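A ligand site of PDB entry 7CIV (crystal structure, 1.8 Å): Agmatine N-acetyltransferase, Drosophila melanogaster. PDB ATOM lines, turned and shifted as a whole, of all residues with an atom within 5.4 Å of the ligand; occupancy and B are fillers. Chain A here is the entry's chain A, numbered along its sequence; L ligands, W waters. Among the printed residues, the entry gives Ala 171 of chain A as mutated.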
ATOM      1  N   HIS A  29     -19.322  27.134  28.029  1.00  0.00           N
ATOM      2  CA  HIS A  29     -20.740  27.442  27.834  1.00  0.00           C
ATOM      3  C   HIS A  29     -21.707  26.325  28.182  1.00  0.00           C
ATOM      4  O   HIS A  29     -22.929  26.543  28.140  1.00  0.00           O
ATOM      5  CB  HIS A  29     -20.961  27.888  26.393  1.00  0.00           C
ATOM      6  CG  HIS A  29     -20.175  29.093  26.008  1.00  0.00           C
ATOM      7  ND1 HIS A  29     -20.227  30.271  26.722  1.00  0.00           N
ATOM      8  CD2 HIS A  29     -19.310  29.310  24.991  1.00  0.00           C
ATOM      9  CE1 HIS A  29     -19.438  31.169  26.161  1.00  0.00           C
ATOM     10  NE2 HIS A  29     -18.871  30.609  25.104  1.00  0.00           N
ATOM     11  N   TYR A  30     -21.213  25.134  28.523  1.00  0.00           N
ATOM     12  CA  TYR A  30     -22.077  24.057  28.988  1.00  0.00           C
ATOM     13  C   TYR A  30     -21.936  23.904  30.497  1.00  0.00           C
ATOM     14  O   TYR A  30     -22.870  24.190  31.249  1.00  0.00           O
ATOM     15  CB  TYR A  30     -21.726  22.747  28.276  1.00  0.00           C
ATOM     16  CG  TYR A  30     -22.444  21.539  28.875  1.00  0.00           C
ATOM     17  CD1 TYR A  30     -23.795  21.344  28.667  1.00  0.00           C
ATOM     18  CD2 TYR A  30     -21.761  20.618  29.672  1.00  0.00           C
ATOM     19  CE1 TYR A  30     -24.466  20.269  29.226  1.00  0.00           C
ATOM     20  CE2 TYR A  30     -22.423  19.521  30.232  1.00  0.00           C
ATOM     21  CZ  TYR A  30     -23.778  19.367  30.008  1.00  0.00           C
ATOM     22  OH  TYR A  30     -24.456  18.294  30.559  1.00  0.00           O
ATOM     23  N   GLU A  33     -23.129  26.530  33.508  1.00  0.00           N
ATOM     24  CA  GLU A  33     -24.552  26.750  33.750  1.00  0.00           C
ATOM     25  C   GLU A  33     -25.366  25.467  33.878  1.00  0.00           C
ATOM     26  O   GLU A  33     -26.561  25.539  34.200  1.00  0.00           O
ATOM     27  CB  GLU A  33     -25.168  27.594  32.636  1.00  0.00           C
ATOM     28  CG  GLU A  33     -24.602  28.989  32.526  1.00  0.00           C
ATOM     29  CD  GLU A  33     -24.891  29.581  31.172  1.00  0.00           C
ATOM     30  OE1 GLU A  33     -24.000  29.507  30.295  1.00  0.00           O
ATOM     31  OE2 GLU A  33     -26.014  30.084  30.970  1.00  0.00           O
ATOM     32  N   GLU A  34     -24.791  24.318  33.565  1.00  0.00           N
ATOM     33  CA  GLU A  34     -25.517  23.068  33.681  1.00  0.00           C
ATOM     34  C   GLU A  34     -25.898  22.857  35.152  1.00  0.00           C
ATOM     35  O   GLU A  34     -25.038  22.972  36.032  1.00  0.00           O
ATOM     36  CB  GLU A  34     -24.646  21.918  33.152  1.00  0.00           C
ATOM     37  CG  GLU A  34     -25.405  20.622  32.867  1.00  0.00           C
ATOM     38  CD  GLU A  34     -25.698  19.872  34.136  1.00  0.00           C
ATOM     39  OE1 GLU A  34     -24.770  19.789  34.973  1.00  0.00           O
ATOM     40  OE2 GLU A  34     -26.835  19.380  34.304  1.00  0.00           O
ATOM     41  N   PRO A  35     -27.175  22.588  35.460  1.00  0.00           N
ATOM     42  CA  PRO A  35     -27.591  22.640  36.871  1.00  0.00           C
ATOM     43  C   PRO A  35     -26.912  21.618  37.769  1.00  0.00           C
ATOM     44  O   PRO A  35     -26.638  21.946  38.931  1.00  0.00           O
ATOM     45  CB  PRO A  35     -29.116  22.419  36.793  1.00  0.00           C
ATOM     46  CG  PRO A  35     -29.490  22.968  35.473  1.00  0.00           C
ATOM     47  CD  PRO A  35     -28.338  22.576  34.550  1.00  0.00           C
ATOM     48  N   VAL A 128     -28.982  11.451  24.997  1.00  0.00           N
ATOM     49  CA  VAL A 128     -28.280  12.736  24.892  1.00  0.00           C
ATOM     50  C   VAL A 128     -27.732  13.101  26.255  1.00  0.00           C
ATOM     51  O   VAL A 128     -28.488  13.291  27.223  1.00  0.00           O
ATOM     52  CB  VAL A 128     -29.205  13.830  24.347  1.00  0.00           C
ATOM     53  CG1 VAL A 128     -28.521  15.201  24.423  1.00  0.00           C
ATOM     54  CG2 VAL A 128     -29.589  13.512  22.916  1.00  0.00           C
ATOM     55  N   HIS A 129     -26.412  13.220  26.348  1.00  0.00           N
ATOM     56  CA  HIS A 129     -25.749  13.459  27.629  1.00  0.00           C
ATOM     57  C   HIS A 129     -25.538  14.928  27.931  1.00  0.00           C
ATOM     58  O   HIS A 129     -25.482  15.301  29.102  1.00  0.00           O
ATOM     59  CB  HIS A 129     -24.393  12.745  27.657  1.00  0.00           C
ATOM     60  CG  HIS A 129     -24.501  11.256  27.553  1.00  0.00           C
ATOM     61  ND1 HIS A 129     -24.988  10.482  28.587  1.00  0.00           N
ATOM     62  CD2 HIS A 129     -24.212  10.395  26.550  1.00  0.00           C
ATOM     63  CE1 HIS A 129     -24.983   9.214  28.225  1.00  0.00           C
ATOM     64  NE2 HIS A 129     -24.522   9.134  26.992  1.00  0.00           N
ATOM     65  N   ALA A 130     -25.410  15.764  26.904  1.00  0.00           N
ATOM     66  CA  ALA A 130     -25.038  17.159  27.070  1.00  0.00           C
ATOM     67  C   ALA A 130     -25.512  17.933  25.861  1.00  0.00           C
ATOM     68  O   ALA A 130     -25.389  17.463  24.728  1.00  0.00           O
ATOM     69  CB  ALA A 130     -23.524  17.341  27.226  1.00  0.00           C
ATOM     70  N   LEU A 131     -26.033  19.132  26.114  1.00  0.00           N
ATOM     71  CA  LEU A 131     -26.446  20.048  25.071  1.00  0.00           C
ATOM     72  C   LEU A 131     -26.126  21.455  25.559  1.00  0.00           C
ATOM     73  O   LEU A 131     -26.565  21.846  26.658  1.00  0.00           O
ATOM     74  CB  LEU A 131     -27.934  19.900  24.747  1.00  0.00           C
ATOM     75  CG  LEU A 131     -28.494  20.876  23.699  1.00  0.00           C
ATOM     76  CD1 LEU A 131     -28.003  20.524  22.299  1.00  0.00           C
ATOM     77  CD2 LEU A 131     -30.006  20.878  23.759  1.00  0.00           C
ATOM     78  N   GLY A 132     -25.343  22.189  24.774  1.00  0.00           N
ATOM     79  CA  GLY A 132     -24.976  23.545  25.155  1.00  0.00           C
ATOM     80  C   GLY A 132     -24.960  24.495  23.976  1.00  0.00           C
ATOM     81  O   GLY A 132     -24.571  24.104  22.879  1.00  0.00           O
ATOM     82  N   VAL A 133     -25.381  25.735  24.197  1.00  0.00           N
ATOM     83  CA  VAL A 133     -25.351  26.765  23.160  1.00  0.00           C
ATOM     84  C   VAL A 133     -24.684  28.020  23.714  1.00  0.00           C
ATOM     85  O   VAL A 133     -24.998  28.467  24.825  1.00  0.00           O
ATOM     86  CB  VAL A 133     -26.769  27.081  22.623  1.00  0.00           C
ATOM     87  CG1 VAL A 133     -26.731  28.252  21.639  1.00  0.00           C
ATOM     88  CG2 VAL A 133     -27.388  25.846  21.946  1.00  0.00           C
ATOM     89  N   ASP A 134     -23.741  28.589  22.945  1.00  0.00           N
ATOM     90  CA  ASP A 134     -23.142  29.877  23.276  1.00  0.00           C
ATOM     91  C   ASP A 134     -24.244  30.869  23.654  1.00  0.00           C
ATOM     92  O   ASP A 134     -25.238  31.006  22.915  1.00  0.00           O
ATOM     93  CB  ASP A 134     -22.319  30.387  22.082  1.00  0.00           C
ATOM     94  CG  ASP A 134     -21.548  31.691  22.398  1.00  0.00           C
ATOM     95  OD1 ASP A 134     -22.146  32.642  22.927  1.00  0.00           O
ATOM     96  OD2 ASP A 134     -20.334  31.759  22.095  1.00  0.00           O
ATOM     97  N   LEU A 137     -25.886  33.129  21.155  1.00  0.00           N
ATOM     98  CA  LEU A 137     -26.670  32.528  20.091  1.00  0.00           C
ATOM     99  C   LEU A 137     -27.871  31.755  20.608  1.00  0.00           C
ATOM    100  O   LEU A 137     -28.488  31.009  19.839  1.00  0.00           O
ATOM    101  CB  LEU A 137     -25.805  31.613  19.221  1.00  0.00           C
ATOM    102  CG  LEU A 137     -24.911  32.395  18.255  1.00  0.00           C
ATOM    103  CD1 LEU A 137     -24.360  31.461  17.243  1.00  0.00           C
ATOM    104  CD2 LEU A 137     -25.692  33.510  17.577  1.00  0.00           C
ATOM    105  N   ARG A 138     -28.239  31.918  21.871  1.00  0.00           N
ATOM    106  CA  ARG A 138     -29.437  31.298  22.384  1.00  0.00           C
ATOM    107  C   ARG A 138     -30.666  32.004  21.836  1.00  0.00           C
ATOM    108  O   ARG A 138     -30.640  33.201  21.527  1.00  0.00           O
ATOM    109  CB  ARG A 138     -29.421  31.302  23.924  1.00  0.00           C
ATOM    110  CG  ARG A 138     -28.414  30.304  24.497  1.00  0.00           C
ATOM    111  CD  ARG A 138     -28.219  30.415  26.005  1.00  0.00           C
ATOM    112  NE  ARG A 138     -27.047  29.638  26.419  1.00  0.00           N
ATOM    113  CZ  ARG A 138     -26.518  29.679  27.633  1.00  0.00           C
ATOM    114  NH1 ARG A 138     -27.064  30.449  28.566  1.00  0.00           N
ATOM    115  NH2 ARG A 138     -25.457  28.924  27.921  1.00  0.00           N
ATOM    116  N   GLY A 139     -31.759  31.256  21.688  1.00  0.00           N
ATOM    117  CA  GLY A 139     -32.965  31.805  21.112  1.00  0.00           C
ATOM    118  C   GLY A 139     -33.144  31.548  19.646  1.00  0.00           C
ATOM    119  O   GLY A 139     -34.188  31.911  19.095  1.00  0.00           O
ATOM    120  N   ARG A 140     -32.153  30.924  19.003  1.00  0.00           N
ATOM    121  CA  ARG A 140     -32.156  30.693  17.571  1.00  0.00           C
ATOM    122  C   ARG A 140     -32.442  29.239  17.252  1.00  0.00           C
ATOM    123  O   ARG A 140     -32.261  28.829  16.096  1.00  0.00           O
ATOM    124  CB  ARG A 140     -30.811  31.130  16.981  1.00  0.00           C
ATOM    125  CG  ARG A 140     -30.523  32.624  17.163  1.00  0.00           C
ATOM    126  CD  ARG A 140     -29.351  33.085  16.303  1.00  0.00           C
ATOM    127  NE  ARG A 140     -29.469  32.602  14.922  1.00  0.00           N
ATOM    128  CZ  ARG A 140     -28.524  32.761  13.987  1.00  0.00           C
ATOM    129  NH1 ARG A 140     -27.394  33.390  14.292  1.00  0.00           N
ATOM    130  NH2 ARG A 140     -28.719  32.284  12.768  1.00  0.00           N
ATOM    131  N   ASN A 141     -32.878  28.466  18.235  1.00  0.00           N
ATOM    132  CA  ASN A 141     -33.160  27.042  18.059  1.00  0.00           C
ATOM    133  C   ASN A 141     -31.938  26.301  17.524  1.00  0.00           C
ATOM    134  O   ASN A 141     -32.050  25.350  16.741  1.00  0.00           O
ATOM    135  CB  ASN A 141     -34.377  26.847  17.161  1.00  0.00           C
ATOM    136  CG  ASN A 141     -35.083  25.543  17.444  1.00  0.00           C
ATOM    137  OD1 ASN A 141     -35.580  25.303  18.555  1.00  0.00           O
ATOM    138  ND2 ASN A 141     -35.126  24.689  16.432  1.00  0.00           N
ATOM    139  N   LEU A 142     -30.736  26.732  17.921  1.00  0.00           N
ATOM    140  CA  LEU A 142     -29.568  25.890  17.668  1.00  0.00           C
ATOM    141  C   LEU A 142     -29.672  24.599  18.456  1.00  0.00           C
ATOM    142  O   LEU A 142     -29.327  23.526  17.950  1.00  0.00           O
ATOM    143  CB  LEU A 142     -28.290  26.642  18.030  1.00  0.00           C
ATOM    144  CG  LEU A 142     -27.836  27.800  17.130  1.00  0.00           C
ATOM    145  CD1 LEU A 142     -26.440  28.253  17.521  1.00  0.00           C
ATOM    146  CD2 LEU A 142     -27.854  27.368  15.667  1.00  0.00           C
ATOM    147  N   GLY A 143     -30.164  24.675  19.699  1.00  0.00           N
ATOM    148  CA  GLY A 143     -30.382  23.458  20.471  1.00  0.00           C
ATOM    149  C   GLY A 143     -31.306  22.490  19.765  1.00  0.00           C
ATOM    150  O   GLY A 143     -31.021  21.288  19.655  1.00  0.00           O
ATOM    151  N   GLY A 144     -32.417  22.999  19.237  1.00  0.00           N
ATOM    152  CA  GLY A 144     -33.353  22.124  18.542  1.00  0.00           C
ATOM    153  C   GLY A 144     -32.753  21.475  17.305  1.00  0.00           C
ATOM    154  O   GLY A 144     -32.991  20.287  17.041  1.00  0.00           O
ATOM    155  N   VAL A 164     -33.435  11.705  27.073  1.00  0.00           N
ATOM    156  CA  VAL A 164     -32.661  12.856  27.528  1.00  0.00           C
ATOM    157  C   VAL A 164     -33.130  13.276  28.921  1.00  0.00           C
ATOM    158  O   VAL A 164     -34.340  13.370  29.170  1.00  0.00           O
ATOM    159  CB  VAL A 164     -32.767  14.015  26.514  1.00  0.00           C
ATOM    160  CG1 VAL A 164     -34.229  14.476  26.338  1.00  0.00           C
ATOM    161  CG2 VAL A 164     -31.876  15.173  26.918  1.00  0.00           C
ATOM    162  N   ASP A 165     -32.180  13.495  29.837  1.00  0.00           N
ATOM    163  CA  ASP A 165     -32.476  13.991  31.184  1.00  0.00           C
ATOM    164  C   ASP A 165     -32.284  15.503  31.177  1.00  0.00           C
ATOM    165  O   ASP A 165     -31.145  15.996  31.174  1.00  0.00           O
ATOM    166  CB  ASP A 165     -31.579  13.355  32.240  1.00  0.00           C
ATOM    167  CG  ASP A 165     -31.599  11.838  32.203  1.00  0.00           C
ATOM    168  OD1 ASP A 165     -32.690  11.263  32.029  1.00  0.00           O
ATOM    169  OD2 ASP A 165     -30.503  11.228  32.333  1.00  0.00           O
ATOM    170  N   CYS A 166     -33.397  16.240  31.155  1.00  0.00           N
ATOM    171  CA  CYS A 166     -33.373  17.694  31.116  1.00  0.00           C
ATOM    172  C   CYS A 166     -33.204  18.198  32.538  1.00  0.00           C
ATOM    173  O   CYS A 166     -34.176  18.339  33.297  1.00  0.00           O
ATOM    174  CB  CYS A 166     -34.638  18.224  30.455  1.00  0.00           C
ATOM    175  SG  CYS A 166     -34.628  17.866  28.700  1.00  0.00           S
ATOM    176  N   THR A 167     -31.947  18.454  32.904  1.00  0.00           N
ATOM    177  CA  THR A 167     -31.631  18.979  34.229  1.00  0.00           C
ATOM    178  C   THR A 167     -31.982  20.459  34.330  1.00  0.00           C
ATOM    179  O   THR A 167     -32.082  20.995  35.443  1.00  0.00           O
ATOM    180  CB  THR A 167     -30.159  18.762  34.548  1.00  0.00           C
ATOM    181  OG1 THR A 167     -29.365  19.371  33.519  1.00  0.00           O
ATOM    182  CG2 THR A 167     -29.808  17.242  34.619  1.00  0.00           C
ATOM    183  N   SER A 168     -32.186  21.097  33.185  1.00  0.00           N
ATOM    184  CA  SER A 168     -32.447  22.516  33.042  1.00  0.00           C
ATOM    185  C   SER A 168     -33.844  22.737  32.475  1.00  0.00           C
ATOM    186  O   SER A 168     -34.249  22.039  31.536  1.00  0.00           O
ATOM    187  CB  SER A 168     -31.415  23.159  32.089  1.00  0.00           C
ATOM    188  OG  SER A 168     -31.941  24.334  31.503  1.00  0.00           O
ATOM    189  N   TYR A 170     -34.700  25.044  30.585  1.00  0.00           N
ATOM    190  CA  TYR A 170     -34.624  25.481  29.193  1.00  0.00           C
ATOM    191  C   TYR A 170     -34.472  24.302  28.248  1.00  0.00           C
ATOM    192  O   TYR A 170     -34.993  24.351  27.118  1.00  0.00           O
ATOM    193  CB  TYR A 170     -33.482  26.492  29.025  1.00  0.00           C
ATOM    194  CG  TYR A 170     -33.637  27.672  29.935  1.00  0.00           C
ATOM    195  CD1 TYR A 170     -34.601  28.642  29.681  1.00  0.00           C
ATOM    196  CD2 TYR A 170     -32.849  27.803  31.076  1.00  0.00           C
ATOM    197  CE1 TYR A 170     -34.753  29.729  30.536  1.00  0.00           C
ATOM    198  CE2 TYR A 170     -32.995  28.878  31.926  1.00  0.00           C
ATOM    199  CZ  TYR A 170     -33.952  29.837  31.652  1.00  0.00           C
ATOM    200  OH  TYR A 170     -34.099  30.912  32.501  1.00  0.00           O
ATOM    201  N   ALA A 171     -33.789  23.236  28.678  1.00  0.00           N
ATOM    202  CA  ALA A 171     -33.726  22.025  27.873  1.00  0.00           C
ATOM    203  C   ALA A 171     -35.069  21.319  27.823  1.00  0.00           C
ATOM    204  O   ALA A 171     -35.484  20.826  26.771  1.00  0.00           O
ATOM    205  CB  ALA A 171     -32.649  21.084  28.438  1.00  0.00           C
ATOM    206  N   LEU A 174     -37.346  23.158  25.419  1.00  0.00           N
ATOM    207  CA  LEU A 174     -36.930  22.913  24.043  1.00  0.00           C
ATOM    208  C   LEU A 174     -37.433  21.563  23.539  1.00  0.00           C
ATOM    209  O   LEU A 174     -37.980  21.465  22.432  1.00  0.00           O
ATOM    210  CB  LEU A 174     -35.418  23.002  23.945  1.00  0.00           C
ATOM    211  CG  LEU A 174     -34.845  22.267  22.730  1.00  0.00           C
ATOM    212  CD1 LEU A 174     -35.172  23.082  21.465  1.00  0.00           C
ATOM    213  CD2 LEU A 174     -33.352  22.004  22.861  1.00  0.00           C
ATOM    214  N   ARG A 177     -41.089  21.457  22.834  1.00  0.00           N
ATOM    215  CA  ARG A 177     -41.329  22.019  21.501  1.00  0.00           C
ATOM    216  C   ARG A 177     -41.099  20.987  20.403  1.00  0.00           C
ATOM    217  O   ARG A 177     -41.810  20.994  19.388  1.00  0.00           O
ATOM    218  CB  ARG A 177     -40.420  23.232  21.314  1.00  0.00           C
ATOM    219  CG  ARG A 177     -40.706  24.120  20.130  1.00  0.00           C
ATOM    220  CD  ARG A 177     -39.732  25.310  20.145  1.00  0.00           C
ATOM    221  NE  ARG A 177     -39.530  25.807  21.514  1.00  0.00           N
ATOM    222  CZ  ARG A 177     -38.357  26.193  22.017  1.00  0.00           C
ATOM    223  NH1 ARG A 177     -38.273  26.611  23.275  1.00  0.00           N
ATOM    224  NH2 ARG A 177     -37.259  26.139  21.262  1.00  0.00           N
HETATM  225  N1  LIG L   1     -30.994  31.269  30.401  1.00  0.00           N
HETATM  226  C1  LIG L   1     -31.869  32.221  30.101  1.00  0.00           C
HETATM  227  N2  LIG L   1     -32.607  32.192  29.012  1.00  0.00           N
HETATM  228  C2  LIG L   1     -32.476  31.171  28.145  1.00  0.00           C
HETATM  229  C3  LIG L   1     -31.575  30.142  28.401  1.00  0.00           C
HETATM  230  C4  LIG L   1     -30.815  30.228  29.583  1.00  0.00           C
HETATM  231  N3  LIG L   1     -29.877  29.182  29.921  1.00  0.00           N
HETATM  232  N4  LIG L   1     -31.659  29.266  27.391  1.00  0.00           N
HETATM  233  C5  LIG L   1     -32.574  29.734  26.552  1.00  0.00           C
HETATM  234  N5  LIG L   1     -33.093  30.883  27.000  1.00  0.00           N
HETATM  235  C6  LIG L   1     -34.075  31.784  26.368  1.00  0.00           C
HETATM  236  C7  LIG L   1     -35.565  31.329  25.845  1.00  0.00           C
HETATM  237  O1  LIG L   1     -35.804  29.959  25.886  1.00  0.00           O
HETATM  238  C8  LIG L   1     -35.677  31.856  24.663  1.00  0.00           C
HETATM  239  O2  LIG L   1     -35.928  33.235  24.851  1.00  0.00           O
HETATM  240  P1  LIG L   1     -36.466  34.297  23.697  1.00  0.00           P
HETATM  241  O3  LIG L   1     -37.116  35.454  24.400  1.00  0.00           O
HETATM  242  O4  LIG L   1     -35.320  34.825  22.867  1.00  0.00           O
HETATM  243  O5  LIG L   1     -37.470  33.609  22.802  1.00  0.00           O
HETATM  244  C9  LIG L   1     -34.238  31.774  24.113  1.00  0.00           C
HETATM  245  O6  LIG L   1     -33.472  32.339  25.325  1.00  0.00           O
HETATM  246  C10 LIG L   1     -33.779  30.342  23.859  1.00  0.00           C
HETATM  247  O7  LIG L   1     -34.811  29.429  23.652  1.00  0.00           O
HETATM  248  P2  LIG L   1     -34.273  28.040  22.950  1.00  0.00           P
HETATM  249  O8  LIG L   1     -35.320  26.968  23.137  1.00  0.00           O
HETATM  250  O9  LIG L   1     -33.962  28.265  21.484  1.00  0.00           O
HETATM  251  O10 LIG L   1     -32.922  27.596  23.760  1.00  0.00           O
HETATM  252  P3  LIG L   1     -31.443  27.271  23.129  1.00  0.00           P
HETATM  253  O11 LIG L   1     -31.524  26.078  22.222  1.00  0.00           O
HETATM  254  O12 LIG L   1     -30.812  28.445  22.414  1.00  0.00           O
HETATM  255  O13 LIG L   1     -30.582  26.960  24.492  1.00  0.00           O
HETATM  256  C11 LIG L   1     -29.853  25.401  26.046  1.00  0.00           C
HETATM  257  C12 LIG L   1     -31.078  25.953  25.332  1.00  0.00           C
HETATM  258  C13 LIG L   1     -30.288  24.403  27.121  1.00  0.00           C
HETATM  259  C14 LIG L   1     -29.016  24.694  24.974  1.00  0.00           C
HETATM  260  C15 LIG L   1     -29.069  26.571  26.687  1.00  0.00           C
HETATM  261  O14 LIG L   1     -29.826  27.109  27.773  1.00  0.00           O
HETATM  262  C16 LIG L   1     -27.576  26.228  26.984  1.00  0.00           C
HETATM  263  O15 LIG L   1     -26.782  26.184  26.123  1.00  0.00           O
HETATM  264  N6  LIG L   1     -26.804  25.975  28.156  1.00  0.00           N
HETATM  265  C17 LIG L   1     -27.011  25.820  29.539  1.00  0.00           C
HETATM  266  C18 LIG L   1     -26.240  24.501  29.724  1.00  0.00           C
HETATM  267  C19 LIG L   1     -27.345  23.513  30.044  1.00  0.00           C
HETATM  268  O16 LIG L   1     -27.908  23.653  31.086  1.00  0.00           O
HETATM  269  N7  LIG L   1     -27.717  22.522  29.061  1.00  0.00           N
HETATM  270  C20 LIG L   1     -28.818  21.574  29.246  1.00  0.00           C
HETATM  271  C21 LIG L   1     -28.709  20.711  30.494  1.00  0.00           C
HETATM  272  S1  LIG L   1     -29.673  19.191  30.205  1.00  0.00           S
HETATM  273  C22 LIG L   1     -28.789  18.321  28.895  1.00  0.00           C
HETATM  274  O17 LIG L   1     -27.814  18.824  28.473  1.00  0.00           O
HETATM  275  C23 LIG L   1     -29.295  16.982  28.369  1.00  0.00           C
HETATM  276  O   HOH W   1     -30.316  28.840  19.775  1.00  0.00           O
HETATM  277  O   HOH W   2     -29.345  13.824  29.544  1.00  0.00           O
HETATM  278  O   HOH W   3     -35.900  26.652  25.813  1.00  0.00           O
HETATM  279  O   HOH W   4     -29.560  25.716  31.262  1.00  0.00           O
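Water W4 bridges O16 of the ligand (2.6 Å) and OG of Ser 168 (2.8 Å). Water W3 lies within hydrogen-bond range of O8 of the ligand (2.8 Å), O of Tyr 170 (2.8 Å) and NH1 of Arg 177 (3.5 Å). Water W2 bridges O of Val 128 (2.5 Å) and N of Asp 165 (2.9 Å).
The guanidinium group of Arg 138 lies within hydrogen-bond range of an oxygen (O15) of the ligand, 3.5 Å away. The guanidinium group (NH2) of Arg 177 is in salt-bridge range of an oxygen (O8) of the ligand (2.8 Å). N of Leu 131 lies within hydrogen-bond range of O17 of the ligand. An oxygen (O9) of the ligand is in hydrogen-bond range of the backbone NH (N) of Asn 141. N of Gly 139 sits at hydrogen-bond distance from O12 of the ligand, at 3.1 Å. The backbone carbonyl oxygen (O) of Leu 131 is in hydrogen-bond range of a nitrogen (N7) of the ligand (2.7 Å). An oxygen (O15) of the ligand is in hydrogen-bond range of the backbone NH (N) of Val 133 (2.4 Å). A sulfur (S1) of the ligand sits close to the backbone NH of Thr 167 (3.6 Å). N of Gly 143 is in hydrogen-bond range of O11 of the ligand (3.2 Å). The side-chain hydroxyl (OG1) of Thr 167 lies close to a sulfur (S1) of the ligand, 3.3 Å away.
O of Asp 165 lies close to S1 of the ligand. Residues that only touch the ligand: Gly 132, Val 164, Tyr 170, Ala 130, Glu 34, Pro 35, Ser 168, Tyr 30, Glu 33, His 29, Ala 171 and Val 128. Hydrophobic or aromatic side chains within 4 Å of the ligand: Tyr 30, Pro 35, Leu 131, Val 133, Val 164, Tyr 170 and Ala 171. Within 4 Å of the ligand: His 29, Tyr 30, Glu 33, Glu 34, Pro 35, Val 128, Ala 130, Leu 131, Gly 132, Val 133, Arg 138, Gly 139, Asn 141, Gly 143, Val 164, Asp 165, Thr 167, Ser 168, Tyr 170, Ala 171 and Arg 177. The nearest printed residue that does not touch the ligand is Leu 174 (4.05 Å).
NH2 of Arg 177 sits at hydrogen-bond distance from OD1 of Asn 141. OG of Ser 168 is in hydrogen-bond range of N of Tyr 170 (3.0 Å). NH2 of Arg 138 sits at hydrogen-bond distance from O of His 29 (3.5 Å). O of Val 133 lies within hydrogen-bond range of NE of Arg 138 (2.8 Å). The guanidinium group (NH1) of Arg 138 lies within salt-bridge range of the side-chain carboxylate (OE2) of Glu 33, at 2.6 Å. OG1 of Thr 167 is in hydrogen-bond range of OE2 of Glu 34 (2.6 Å). The side-chain hydroxyl (OH) of Tyr 30 lies within hydrogen-bond range of the backbone carbonyl oxygen (O) of His 129 (3.5 Å). The side-chain sulfur (SG) of Cys 166 lies close to the backbone carbonyl oxygen (O) of Ala 171 (3.6 Å).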
